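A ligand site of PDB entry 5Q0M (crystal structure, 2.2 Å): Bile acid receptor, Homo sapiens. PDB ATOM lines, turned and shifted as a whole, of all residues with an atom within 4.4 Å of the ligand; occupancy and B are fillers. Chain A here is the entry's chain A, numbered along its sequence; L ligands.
The side-chain hydroxyl (OG1) of Thr 31 lies within hydrogen-bond range of an oxygen (O2) of the ligand, at 3.3 Å.
O6 of the ligand is in hydrogen-bond range of N of Met 26.
The side-chain hydroxyl of Thr 49 is in hydrogen-bond range of an oxygen (O4) of the ligand (3.0 Å).
An oxygen (O1) of the ligand lies within salt-bridge range of the guanidinium group (NH2) of Arg 92, at 3.2 Å.
The backbone carbonyl oxygen (O) of Phe 45 is in hydrogen-bond range of the side-chain hydroxyl (OG1) of Thr 49, 2.9 Å away.
The backbone NH (N) of Leu 101 is in hydrogen-bond range of the backbone carbonyl oxygen (O) of Ile 96 (3.1 Å).
The side-chain hydroxyl (OH) of Tyr 122 sits at hydrogen-bond distance from a ring nitrogen (ND1) of His 208.
The backbone carbonyl oxygen (O) of Met 89 sits at hydrogen-bond distance from the side-chain hydroxyl (OG) of Ser 93, 2.8 Å away.
OE1 of Gln 24 lies within hydrogen-bond range of NE of Arg 92 (3.2 Å).
OG of Ser 93 is in hydrogen-bond range of OH of Tyr 130 (2.9 Å).
The side-chain hydroxyl (OG) of Ser 93 lies within hydrogen-bond range of the backbone carbonyl oxygen (O) of Phe 90 (2.9 Å).
Arg 25 touches the ligand.
Phe 45 touches the ligand.
CD2 of Leu 48 touches C8 of the ligand, 3.7 Å away.
Met 51 touches the ligand.
Met 89 touches the ligand.
Ser 93 touches the ligand (CB to C20, 3.9 Å).
Ile 96 touches the ligand.
Leu 101 touches the ligand.
CD1 of Leu 109 touches C27 of the ligand (3.7 Å).
Ile 118 touches the ligand.
Tyr 122 touches the ligand.
OH of Tyr 130 touches C9 of the ligand, 3.7 Å away.
CE1 of His 208 touches C11 of the ligand, at 3.6 Å.
Phe 222 touches the ligand (CE2 to O4, 3.9 Å).
Hydrophobic or aromatic side chains within 4 Å of the ligand: Met 26, Phe 45, Leu 48, Met 51, Met 89, Ile 96, Leu 101, Leu 109, Ile 118, Tyr 122, His 208 and Phe 222.
Within 4 Å of the ligand: Arg 25, Met 26, Thr 31, Phe 45, Leu 48, Thr 49, Met 51, Met 89, Arg 92, Ser 93, Ile 96, Leu 101, Leu 109, Ile 118, Tyr 122, Tyr 130, His 208 and Phe 222.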
ATOM      1  N   GLN A  24     -11.724   8.862  -8.603  1.00  0.00           N
ATOM      2  CA  GLN A  24     -10.920   8.208  -9.630  1.00  0.00           C
ATOM      3  C   GLN A  24     -10.813   6.718  -9.308  1.00  0.00           C
ATOM      4  O   GLN A  24     -10.468   6.339  -8.178  1.00  0.00           O
ATOM      5  CB  GLN A  24      -9.525   8.823  -9.726  1.00  0.00           C
ATOM      6  CG  GLN A  24      -9.454  10.350  -9.714  1.00  0.00           C
ATOM      7  CD  GLN A  24      -8.028  10.895  -9.902  1.00  0.00           C
ATOM      8  OE1 GLN A  24      -7.038  10.186  -9.708  1.00  0.00           O
ATOM      9  NE2 GLN A  24      -7.921  12.154 -10.278  1.00  0.00           N
ATOM     10  N   ARG A  25     -11.122   5.882 -10.291  1.00  0.00           N
ATOM     11  CA  ARG A  25     -10.862   4.457 -10.206  1.00  0.00           C
ATOM     12  C   ARG A  25     -10.517   3.946 -11.605  1.00  0.00           C
ATOM     13  O   ARG A  25     -11.070   4.415 -12.598  1.00  0.00           O
ATOM     14  CB  ARG A  25     -12.061   3.683  -9.638  1.00  0.00           C
ATOM     15  CG  ARG A  25     -11.973   2.159  -9.803  1.00  0.00           C
ATOM     16  CD  ARG A  25     -13.253   1.552 -10.412  1.00  0.00           C
ATOM     17  NE  ARG A  25     -13.590   2.094 -11.726  1.00  0.00           N
ATOM     18  CZ  ARG A  25     -14.504   1.575 -12.555  1.00  0.00           C
ATOM     19  NH1 ARG A  25     -14.750   2.150 -13.731  1.00  0.00           N
ATOM     20  NH2 ARG A  25     -15.163   0.482 -12.208  1.00  0.00           N
ATOM     21  N   MET A  26      -9.600   3.037 -11.661  1.00  0.00           N
ATOM     22  CA  MET A  26      -9.357   2.372 -12.928  1.00  0.00           C
ATOM     23  C   MET A  26     -10.017   0.998 -12.938  1.00  0.00           C
ATOM     24  O   MET A  26      -9.949   0.258 -11.949  1.00  0.00           O
ATOM     25  CB  MET A  26      -7.865   2.230 -13.201  1.00  0.00           C
ATOM     26  CG  MET A  26      -7.571   2.071 -14.666  1.00  0.00           C
ATOM     27  SD  MET A  26      -6.013   1.301 -15.008  1.00  0.00           S
ATOM     28  CE  MET A  26      -5.078   2.744 -15.476  1.00  0.00           C
ATOM     29  N   THR A  31      -6.846  -3.592 -15.113  1.00  0.00           N
ATOM     30  CA  THR A  31      -5.904  -4.148 -14.140  1.00  0.00           C
ATOM     31  C   THR A  31      -5.648  -5.631 -14.343  1.00  0.00           C
ATOM     32  O   THR A  31      -4.519  -6.104 -14.203  1.00  0.00           O
ATOM     33  CB  THR A  31      -6.431  -3.877 -12.724  1.00  0.00           C
ATOM     34  OG1 THR A  31      -6.250  -2.496 -12.425  1.00  0.00           O
ATOM     35  CG2 THR A  31      -5.699  -4.728 -11.689  1.00  0.00           C
ATOM     36  N   PHE A  45       3.348  -2.822 -24.936  1.00  0.00           N
ATOM     37  CA  PHE A  45       3.068  -1.437 -25.277  1.00  0.00           C
ATOM     38  C   PHE A  45       1.580  -1.220 -25.480  1.00  0.00           C
ATOM     39  O   PHE A  45       1.031  -0.185 -25.095  1.00  0.00           O
ATOM     40  CB  PHE A  45       3.871  -1.012 -26.491  1.00  0.00           C
ATOM     41  CG  PHE A  45       3.818   0.481 -26.766  1.00  0.00           C
ATOM     42  CD1 PHE A  45       4.664   1.362 -26.102  1.00  0.00           C
ATOM     43  CD2 PHE A  45       2.919   0.979 -27.689  1.00  0.00           C
ATOM     44  CE1 PHE A  45       4.620   2.712 -26.365  1.00  0.00           C
ATOM     45  CE2 PHE A  45       2.865   2.351 -27.958  1.00  0.00           C
ATOM     46  CZ  PHE A  45       3.720   3.213 -27.307  1.00  0.00           C
ATOM     47  N   LEU A  48      -0.059  -0.974 -21.983  1.00  0.00           N
ATOM     48  CA  LEU A  48       0.300   0.271 -21.320  1.00  0.00           C
ATOM     49  C   LEU A  48      -0.389   1.440 -21.988  1.00  0.00           C
ATOM     50  O   LEU A  48      -0.757   2.420 -21.330  1.00  0.00           O
ATOM     51  CB  LEU A  48       1.818   0.449 -21.315  1.00  0.00           C
ATOM     52  CG  LEU A  48       2.558  -0.625 -20.528  1.00  0.00           C
ATOM     53  CD1 LEU A  48       4.029  -0.561 -20.836  1.00  0.00           C
ATOM     54  CD2 LEU A  48       2.304  -0.394 -19.078  1.00  0.00           C
ATOM     55  N   THR A  49      -0.594   1.355 -23.305  1.00  0.00           N
ATOM     56  CA  THR A  49      -1.329   2.390 -24.016  1.00  0.00           C
ATOM     57  C   THR A  49      -2.800   2.413 -23.587  1.00  0.00           C
ATOM     58  O   THR A  49      -3.438   3.473 -23.585  1.00  0.00           O
ATOM     59  CB  THR A  49      -1.189   2.147 -25.519  1.00  0.00           C
ATOM     60  OG1 THR A  49       0.168   2.415 -25.915  1.00  0.00           O
ATOM     61  CG2 THR A  49      -2.069   3.058 -26.264  1.00  0.00           C
ATOM     62  N   MET A  51      -3.920   1.564 -20.470  1.00  0.00           N
ATOM     63  CA  MET A  51      -3.920   2.208 -19.162  1.00  0.00           C
ATOM     64  C   MET A  51      -3.810   3.720 -19.287  1.00  0.00           C
ATOM     65  O   MET A  51      -4.528   4.451 -18.590  1.00  0.00           O
ATOM     66  CB  MET A  51      -2.787   1.663 -18.314  1.00  0.00           C
ATOM     67  CG  MET A  51      -2.795   0.192 -18.304  1.00  0.00           C
ATOM     68  SD  MET A  51      -1.671  -0.369 -17.062  1.00  0.00           S
ATOM     69  CE  MET A  51      -2.351   0.478 -15.638  1.00  0.00           C
ATOM     70  N   ALA A  52      -2.897   4.202 -20.138  1.00  0.00           N
ATOM     71  CA  ALA A  52      -2.794   5.651 -20.330  1.00  0.00           C
ATOM     72  C   ALA A  52      -4.083   6.225 -20.871  1.00  0.00           C
ATOM     73  O   ALA A  52      -4.507   7.303 -20.449  1.00  0.00           O
ATOM     74  CB  ALA A  52      -1.629   5.986 -21.269  1.00  0.00           C
ATOM     75  N   MET A  89      -0.568  12.177 -15.526  1.00  0.00           N
ATOM     76  CA  MET A  89      -0.515  10.724 -15.509  1.00  0.00           C
ATOM     77  C   MET A  89       0.603  10.243 -14.611  1.00  0.00           C
ATOM     78  O   MET A  89       0.430   9.292 -13.841  1.00  0.00           O
ATOM     79  CB  MET A  89      -0.321  10.176 -16.911  1.00  0.00           C
ATOM     80  CG  MET A  89      -1.412  10.590 -17.848  1.00  0.00           C
ATOM     81  SD  MET A  89      -1.351   9.593 -19.333  1.00  0.00           S
ATOM     82  CE  MET A  89       0.366   9.802 -19.724  1.00  0.00           C
ATOM     83  N   PHE A  90       1.776  10.874 -14.718  1.00  0.00           N
ATOM     84  CA  PHE A  90       2.915  10.437 -13.938  1.00  0.00           C
ATOM     85  C   PHE A  90       2.714  10.735 -12.464  1.00  0.00           C
ATOM     86  O   PHE A  90       3.081   9.913 -11.609  1.00  0.00           O
ATOM     87  CB  PHE A  90       4.214  11.057 -14.491  1.00  0.00           C
ATOM     88  CG  PHE A  90       4.750  10.321 -15.719  1.00  0.00           C
ATOM     89  CD1 PHE A  90       5.142   8.982 -15.623  1.00  0.00           C
ATOM     90  CD2 PHE A  90       4.853  10.943 -16.936  1.00  0.00           C
ATOM     91  CE1 PHE A  90       5.608   8.284 -16.730  1.00  0.00           C
ATOM     92  CE2 PHE A  90       5.328  10.257 -18.063  1.00  0.00           C
ATOM     93  CZ  PHE A  90       5.710   8.917 -17.957  1.00  0.00           C
ATOM     94  N   ARG A  92      -0.154  10.780 -10.915  1.00  0.00           N
ATOM     95  CA  ARG A  92      -1.151   9.839 -10.434  1.00  0.00           C
ATOM     96  C   ARG A  92      -0.559   8.455 -10.328  1.00  0.00           C
ATOM     97  O   ARG A  92      -0.780   7.761  -9.332  1.00  0.00           O
ATOM     98  CB  ARG A  92      -2.349   9.823 -11.373  1.00  0.00           C
ATOM     99  CG  ARG A  92      -3.389   8.771 -11.043  1.00  0.00           C
ATOM    100  CD  ARG A  92      -3.907   8.877  -9.597  1.00  0.00           C
ATOM    101  NE  ARG A  92      -4.931   7.861  -9.324  1.00  0.00           N
ATOM    102  CZ  ARG A  92      -5.617   7.745  -8.195  1.00  0.00           C
ATOM    103  NH1 ARG A  92      -5.387   8.570  -7.187  1.00  0.00           N
ATOM    104  NH2 ARG A  92      -6.522   6.783  -8.066  1.00  0.00           N
ATOM    105  N   SER A  93       0.200   8.051 -11.333  1.00  0.00           N
ATOM    106  CA  SER A  93       0.830   6.742 -11.272  1.00  0.00           C
ATOM    107  C   SER A  93       1.832   6.679 -10.135  1.00  0.00           C
ATOM    108  O   SER A  93       1.969   5.635  -9.490  1.00  0.00           O
ATOM    109  CB  SER A  93       1.493   6.419 -12.613  1.00  0.00           C
ATOM    110  OG  SER A  93       2.379   7.430 -12.997  1.00  0.00           O
ATOM    111  N   ILE A  96       0.245   5.704  -7.057  1.00  0.00           N
ATOM    112  CA  ILE A  96      -0.200   4.318  -7.004  1.00  0.00           C
ATOM    113  C   ILE A  96       0.962   3.367  -6.750  1.00  0.00           C
ATOM    114  O   ILE A  96       0.841   2.433  -5.961  1.00  0.00           O
ATOM    115  CB  ILE A  96      -0.968   3.949  -8.290  1.00  0.00           C
ATOM    116  CG1 ILE A  96      -2.284   4.696  -8.313  1.00  0.00           C
ATOM    117  CG2 ILE A  96      -1.202   2.482  -8.353  1.00  0.00           C
ATOM    118  CD1 ILE A  96      -2.560   5.327  -9.632  1.00  0.00           C
ATOM    119  N   LEU A 101      -0.013  -0.320  -4.895  1.00  0.00           N
ATOM    120  CA  LEU A 101       0.362  -1.584  -5.527  1.00  0.00           C
ATOM    121  C   LEU A 101       1.324  -2.380  -4.654  1.00  0.00           C
ATOM    122  O   LEU A 101       2.330  -1.831  -4.192  1.00  0.00           O
ATOM    123  CB  LEU A 101       1.012  -1.321  -6.879  1.00  0.00           C
ATOM    124  CG  LEU A 101       0.183  -1.097  -8.142  1.00  0.00           C
ATOM    125  CD1 LEU A 101       1.112  -1.047  -9.359  1.00  0.00           C
ATOM    126  CD2 LEU A 101      -0.877  -2.171  -8.317  1.00  0.00           C
ATOM    127  N   LEU A 109       4.072  -5.043 -13.680  1.00  0.00           N
ATOM    128  CA  LEU A 109       3.886  -3.774 -14.345  1.00  0.00           C
ATOM    129  C   LEU A 109       5.220  -3.194 -14.824  1.00  0.00           C
ATOM    130  O   LEU A 109       5.373  -2.810 -16.002  1.00  0.00           O
ATOM    131  CB  LEU A 109       3.160  -2.841 -13.392  1.00  0.00           C
ATOM    132  CG  LEU A 109       2.672  -1.518 -13.947  1.00  0.00           C
ATOM    133  CD1 LEU A 109       1.982  -1.782 -15.278  1.00  0.00           C
ATOM    134  CD2 LEU A 109       1.768  -0.842 -12.919  1.00  0.00           C
ATOM    135  N   ILE A 113       6.755  -2.458 -18.521  1.00  0.00           N
ATOM    136  CA  ILE A 113       7.222  -1.144 -18.918  1.00  0.00           C
ATOM    137  C   ILE A 113       8.618  -1.236 -19.521  1.00  0.00           C
ATOM    138  O   ILE A 113       8.894  -0.657 -20.575  1.00  0.00           O
ATOM    139  CB  ILE A 113       7.198  -0.174 -17.722  1.00  0.00           C
ATOM    140  CG1 ILE A 113       5.758   0.166 -17.339  1.00  0.00           C
ATOM    141  CG2 ILE A 113       7.918   1.081 -18.085  1.00  0.00           C
ATOM    142  CD1 ILE A 113       5.661   1.109 -16.161  1.00  0.00           C
ATOM    143  N   ILE A 118      10.465   1.015 -25.236  1.00  0.00           N
ATOM    144  CA  ILE A 118      10.668   2.380 -24.799  1.00  0.00           C
ATOM    145  C   ILE A 118      12.085   2.468 -24.262  1.00  0.00           C
ATOM    146  O   ILE A 118      12.581   1.502 -23.666  1.00  0.00           O
ATOM    147  CB  ILE A 118       9.622   2.774 -23.743  1.00  0.00           C
ATOM    148  CG1 ILE A 118       8.247   2.798 -24.392  1.00  0.00           C
ATOM    149  CG2 ILE A 118       9.883   4.155 -23.198  1.00  0.00           C
ATOM    150  CD1 ILE A 118       7.139   2.812 -23.427  1.00  0.00           C
ATOM    151  N   TYR A 122      13.847   7.161 -21.111  1.00  0.00           N
ATOM    152  CA  TYR A 122      12.554   7.451 -20.503  1.00  0.00           C
ATOM    153  C   TYR A 122      12.406   6.699 -19.196  1.00  0.00           C
ATOM    154  O   TYR A 122      11.992   7.275 -18.178  1.00  0.00           O
ATOM    155  CB  TYR A 122      11.430   7.054 -21.473  1.00  0.00           C
ATOM    156  CG  TYR A 122      10.073   7.765 -21.356  1.00  0.00           C
ATOM    157  CD1 TYR A 122       9.197   7.757 -22.430  1.00  0.00           C
ATOM    158  CD2 TYR A 122       9.663   8.402 -20.169  1.00  0.00           C
ATOM    159  CE1 TYR A 122       7.955   8.381 -22.373  1.00  0.00           C
ATOM    160  CE2 TYR A 122       8.413   9.035 -20.100  1.00  0.00           C
ATOM    161  CZ  TYR A 122       7.563   9.011 -21.209  1.00  0.00           C
ATOM    162  OH  TYR A 122       6.329   9.619 -21.184  1.00  0.00           O
ATOM    163  N   MET A 126      11.799   8.042 -15.014  1.00  0.00           N
ATOM    164  CA  MET A 126      10.466   7.665 -14.551  1.00  0.00           C
ATOM    165  C   MET A 126      10.532   6.935 -13.208  1.00  0.00           C
ATOM    166  O   MET A 126       9.922   7.379 -12.231  1.00  0.00           O
ATOM    167  CB  MET A 126       9.789   6.818 -15.629  1.00  0.00           C
ATOM    168  CG  MET A 126       8.649   5.935 -15.180  1.00  0.00           C
ATOM    169  SD  MET A 126       7.534   5.460 -16.523  1.00  0.00           S
ATOM    170  CE  MET A 126       8.495   5.700 -18.002  1.00  0.00           C
ATOM    171  N   TYR A 130       9.367   8.113  -9.325  1.00  0.00           N
ATOM    172  CA  TYR A 130       8.516   7.351  -8.410  1.00  0.00           C
ATOM    173  C   TYR A 130       9.145   7.238  -7.027  1.00  0.00           C
ATOM    174  O   TYR A 130       8.506   7.538  -6.014  1.00  0.00           O
ATOM    175  CB  TYR A 130       8.252   5.963  -8.986  1.00  0.00           C
ATOM    176  CG  TYR A 130       7.326   5.971 -10.186  1.00  0.00           C
ATOM    177  CD1 TYR A 130       6.448   7.034 -10.418  1.00  0.00           C
ATOM    178  CD2 TYR A 130       7.341   4.918 -11.098  1.00  0.00           C
ATOM    179  CE1 TYR A 130       5.598   7.051 -11.542  1.00  0.00           C
ATOM    180  CE2 TYR A 130       6.511   4.914 -12.216  1.00  0.00           C
ATOM    181  CZ  TYR A 130       5.645   5.986 -12.438  1.00  0.00           C
ATOM    182  OH  TYR A 130       4.807   5.979 -13.526  1.00  0.00           O
ATOM    183  N   HIS A 208       8.791  12.153 -23.459  1.00  0.00           N
ATOM    184  CA  HIS A 208       7.595  11.719 -24.176  1.00  0.00           C
ATOM    185  C   HIS A 208       7.608  12.178 -25.627  1.00  0.00           C
ATOM    186  O   HIS A 208       7.147  11.445 -26.516  1.00  0.00           O
ATOM    187  CB  HIS A 208       6.351  12.252 -23.502  1.00  0.00           C
ATOM    188  CG  HIS A 208       5.123  11.544 -23.945  1.00  0.00           C
ATOM    189  ND1 HIS A 208       4.837  10.246 -23.550  1.00  0.00           N
ATOM    190  CD2 HIS A 208       4.138  11.906 -24.796  1.00  0.00           C
ATOM    191  CE1 HIS A 208       3.714   9.863 -24.114  1.00  0.00           C
ATOM    192  NE2 HIS A 208       3.266  10.846 -24.873  1.00  0.00           N
ATOM    193  N   MET A 211       9.804   9.830 -27.424  1.00  0.00           N
ATOM    194  CA  MET A 211       9.147   8.553 -27.665  1.00  0.00           C
ATOM    195  C   MET A 211       8.164   8.669 -28.828  1.00  0.00           C
ATOM    196  O   MET A 211       8.115   7.793 -29.694  1.00  0.00           O
ATOM    197  CB  MET A 211       8.448   8.070 -26.395  1.00  0.00           C
ATOM    198  CG  MET A 211       7.820   6.676 -26.500  1.00  0.00           C
ATOM    199  SD  MET A 211       6.127   6.562 -25.808  1.00  0.00           S
ATOM    200  CE  MET A 211       5.215   6.994 -27.282  1.00  0.00           C
ATOM    201  N   PHE A 222      -1.418   4.022 -31.421  1.00  0.00           N
ATOM    202  CA  PHE A 222      -2.163   4.539 -30.263  1.00  0.00           C
ATOM    203  C   PHE A 222      -3.675   4.465 -30.469  1.00  0.00           C
ATOM    204  O   PHE A 222      -4.163   4.032 -31.512  1.00  0.00           O
ATOM    205  CB  PHE A 222      -1.761   5.987 -29.973  1.00  0.00           C
ATOM    206  CG  PHE A 222      -0.287   6.182 -29.761  1.00  0.00           C
ATOM    207  CD1 PHE A 222       0.582   6.237 -30.841  1.00  0.00           C
ATOM    208  CD2 PHE A 222       0.226   6.305 -28.483  1.00  0.00           C
ATOM    209  CE1 PHE A 222       1.943   6.397 -30.655  1.00  0.00           C
ATOM    210  CE2 PHE A 222       1.588   6.474 -28.286  1.00  0.00           C
ATOM    211  CZ  PHE A 222       2.445   6.512 -29.387  1.00  0.00           C
ATOM    212  N   LEU A 226      -5.697   9.323 -27.250  1.00  0.00           N
ATOM    213  CA  LEU A 226      -4.297   9.699 -27.112  1.00  0.00           C
ATOM    214  C   LEU A 226      -3.813  10.445 -28.344  1.00  0.00           C
ATOM    215  O   LEU A 226      -3.028  11.389 -28.213  1.00  0.00           O
ATOM    216  CB  LEU A 226      -3.442   8.454 -26.869  1.00  0.00           C
ATOM    217  CG  LEU A 226      -3.685   7.770 -25.517  1.00  0.00           C
ATOM    218  CD1 LEU A 226      -2.723   6.580 -25.336  1.00  0.00           C
ATOM    219  CD2 LEU A 226      -3.552   8.761 -24.361  1.00  0.00           C
ATOM    220  N   TRP A 230      -2.220  14.345 -27.979  1.00  0.00           N
ATOM    221  CA  TRP A 230      -0.793  14.504 -28.232  1.00  0.00           C
ATOM    222  C   TRP A 230      -0.453  14.828 -29.705  1.00  0.00           C
ATOM    223  O   TRP A 230       0.719  15.039 -30.013  1.00  0.00           O
ATOM    224  CB  TRP A 230      -0.053  13.230 -27.802  1.00  0.00           C
ATOM    225  CG  TRP A 230      -0.058  12.965 -26.288  1.00  0.00           C
ATOM    226  CD1 TRP A 230      -0.109  13.899 -25.296  1.00  0.00           C
ATOM    227  CD2 TRP A 230      -0.002  11.678 -25.615  1.00  0.00           C
ATOM    228  NE1 TRP A 230      -0.090  13.282 -24.057  1.00  0.00           N
ATOM    229  CE2 TRP A 230      -0.030  11.921 -24.231  1.00  0.00           C
ATOM    230  CE3 TRP A 230       0.067  10.348 -26.059  1.00  0.00           C
ATOM    231  CZ2 TRP A 230       0.021  10.905 -23.284  1.00  0.00           C
ATOM    232  CZ3 TRP A 230       0.109   9.330 -25.101  1.00  0.00           C
ATOM    233  CH2 TRP A 230       0.079   9.617 -23.742  1.00  0.00           C
HETATM  234  C1  LIG L   1      -4.332   2.837 -11.100  1.00  0.00           C
HETATM  235  C2  LIG L   1      -5.445   2.616 -10.283  1.00  0.00           C
HETATM  236  C3  LIG L   1      -5.659   1.359  -9.737  1.00  0.00           C
HETATM  237  C4  LIG L   1      -6.401   3.731  -9.998  1.00  0.00           C
HETATM  238  C5  LIG L   1       2.948   5.987 -19.440  1.00  0.00           C
HETATM  239  C6  LIG L   1       1.388   6.544 -17.427  1.00  0.00           C
HETATM  240  C7  LIG L   1       1.049   4.219 -16.765  1.00  0.00           C
HETATM  241  C8  LIG L   1       2.778   3.222 -18.479  1.00  0.00           C
HETATM  242  C9  LIG L   1       3.419   4.815 -16.706  1.00  0.00           C
HETATM  243  C10 LIG L   1       4.124   5.244 -21.597  1.00  0.00           C
HETATM  244  C11 LIG L   1       3.415   7.653 -21.311  1.00  0.00           C
HETATM  245  C12 LIG L   1       3.575   6.523 -22.283  1.00  0.00           C
HETATM  246  C13 LIG L   1      -4.769   0.323  -9.998  1.00  0.00           C
HETATM  247  C14 LIG L   1      -5.002  -1.027  -9.421  1.00  0.00           C
HETATM  248  C15 LIG L   1       1.896   5.534 -18.453  1.00  0.00           C
HETATM  249  C16 LIG L   1       2.266   4.354 -17.640  1.00  0.00           C
HETATM  250  C17 LIG L   1       3.188   4.846 -20.420  1.00  0.00           C
HETATM  251  C18 LIG L   1       2.485   7.250 -20.176  1.00  0.00           C
HETATM  252  C19 LIG L   1      -3.667   0.544 -10.814  1.00  0.00           C
HETATM  253  C20 LIG L   1       0.697   5.672 -16.375  1.00  0.00           C
HETATM  254  C21 LIG L   1       3.651   3.613 -19.682  1.00  0.00           C
HETATM  255  C22 LIG L   1       1.035   3.290 -15.519  1.00  0.00           C
HETATM  256  C23 LIG L   1       4.198   4.124 -22.643  1.00  0.00           C
HETATM  257  C24 LIG L   1      -3.444   1.792 -11.371  1.00  0.00           C
HETATM  258  C25 LIG L   1       5.552   5.505 -21.081  1.00  0.00           C
HETATM  259  C26 LIG L   1      -0.383   3.293 -14.925  1.00  0.00           C
HETATM  260  C27 LIG L   1       1.465   1.876 -15.819  1.00  0.00           C
HETATM  261  C28 LIG L   1       2.286   6.269 -23.062  1.00  0.00           C
HETATM  262  C29 LIG L   1       2.883   3.887 -23.387  1.00  0.00           C
HETATM  263  C30 LIG L   1      -0.498   2.577 -13.586  1.00  0.00           C
HETATM  264  C31 LIG L   1       2.424   5.154 -24.072  1.00  0.00           C
HETATM  265  C32 LIG L   1      -1.760   2.912 -12.844  1.00  0.00           C
HETATM  266  N1  LIG L   1      -2.282   1.870 -12.179  1.00  0.00           N
HETATM  267  O1  LIG L   1      -6.133   4.863 -10.603  1.00  0.00           O
HETATM  268  O2  LIG L   1      -4.318  -1.990  -9.758  1.00  0.00           O
HETATM  269  O3  LIG L   1      -5.955  -1.101  -8.518  1.00  0.00           O
HETATM  270  O4  LIG L   1       1.175   4.956 -24.736  1.00  0.00           O
HETATM  271  O5  LIG L   1      -2.247   4.051 -12.855  1.00  0.00           O
HETATM  272  O6  LIG L   1      -7.357   3.585  -9.245  1.00  0.00           O
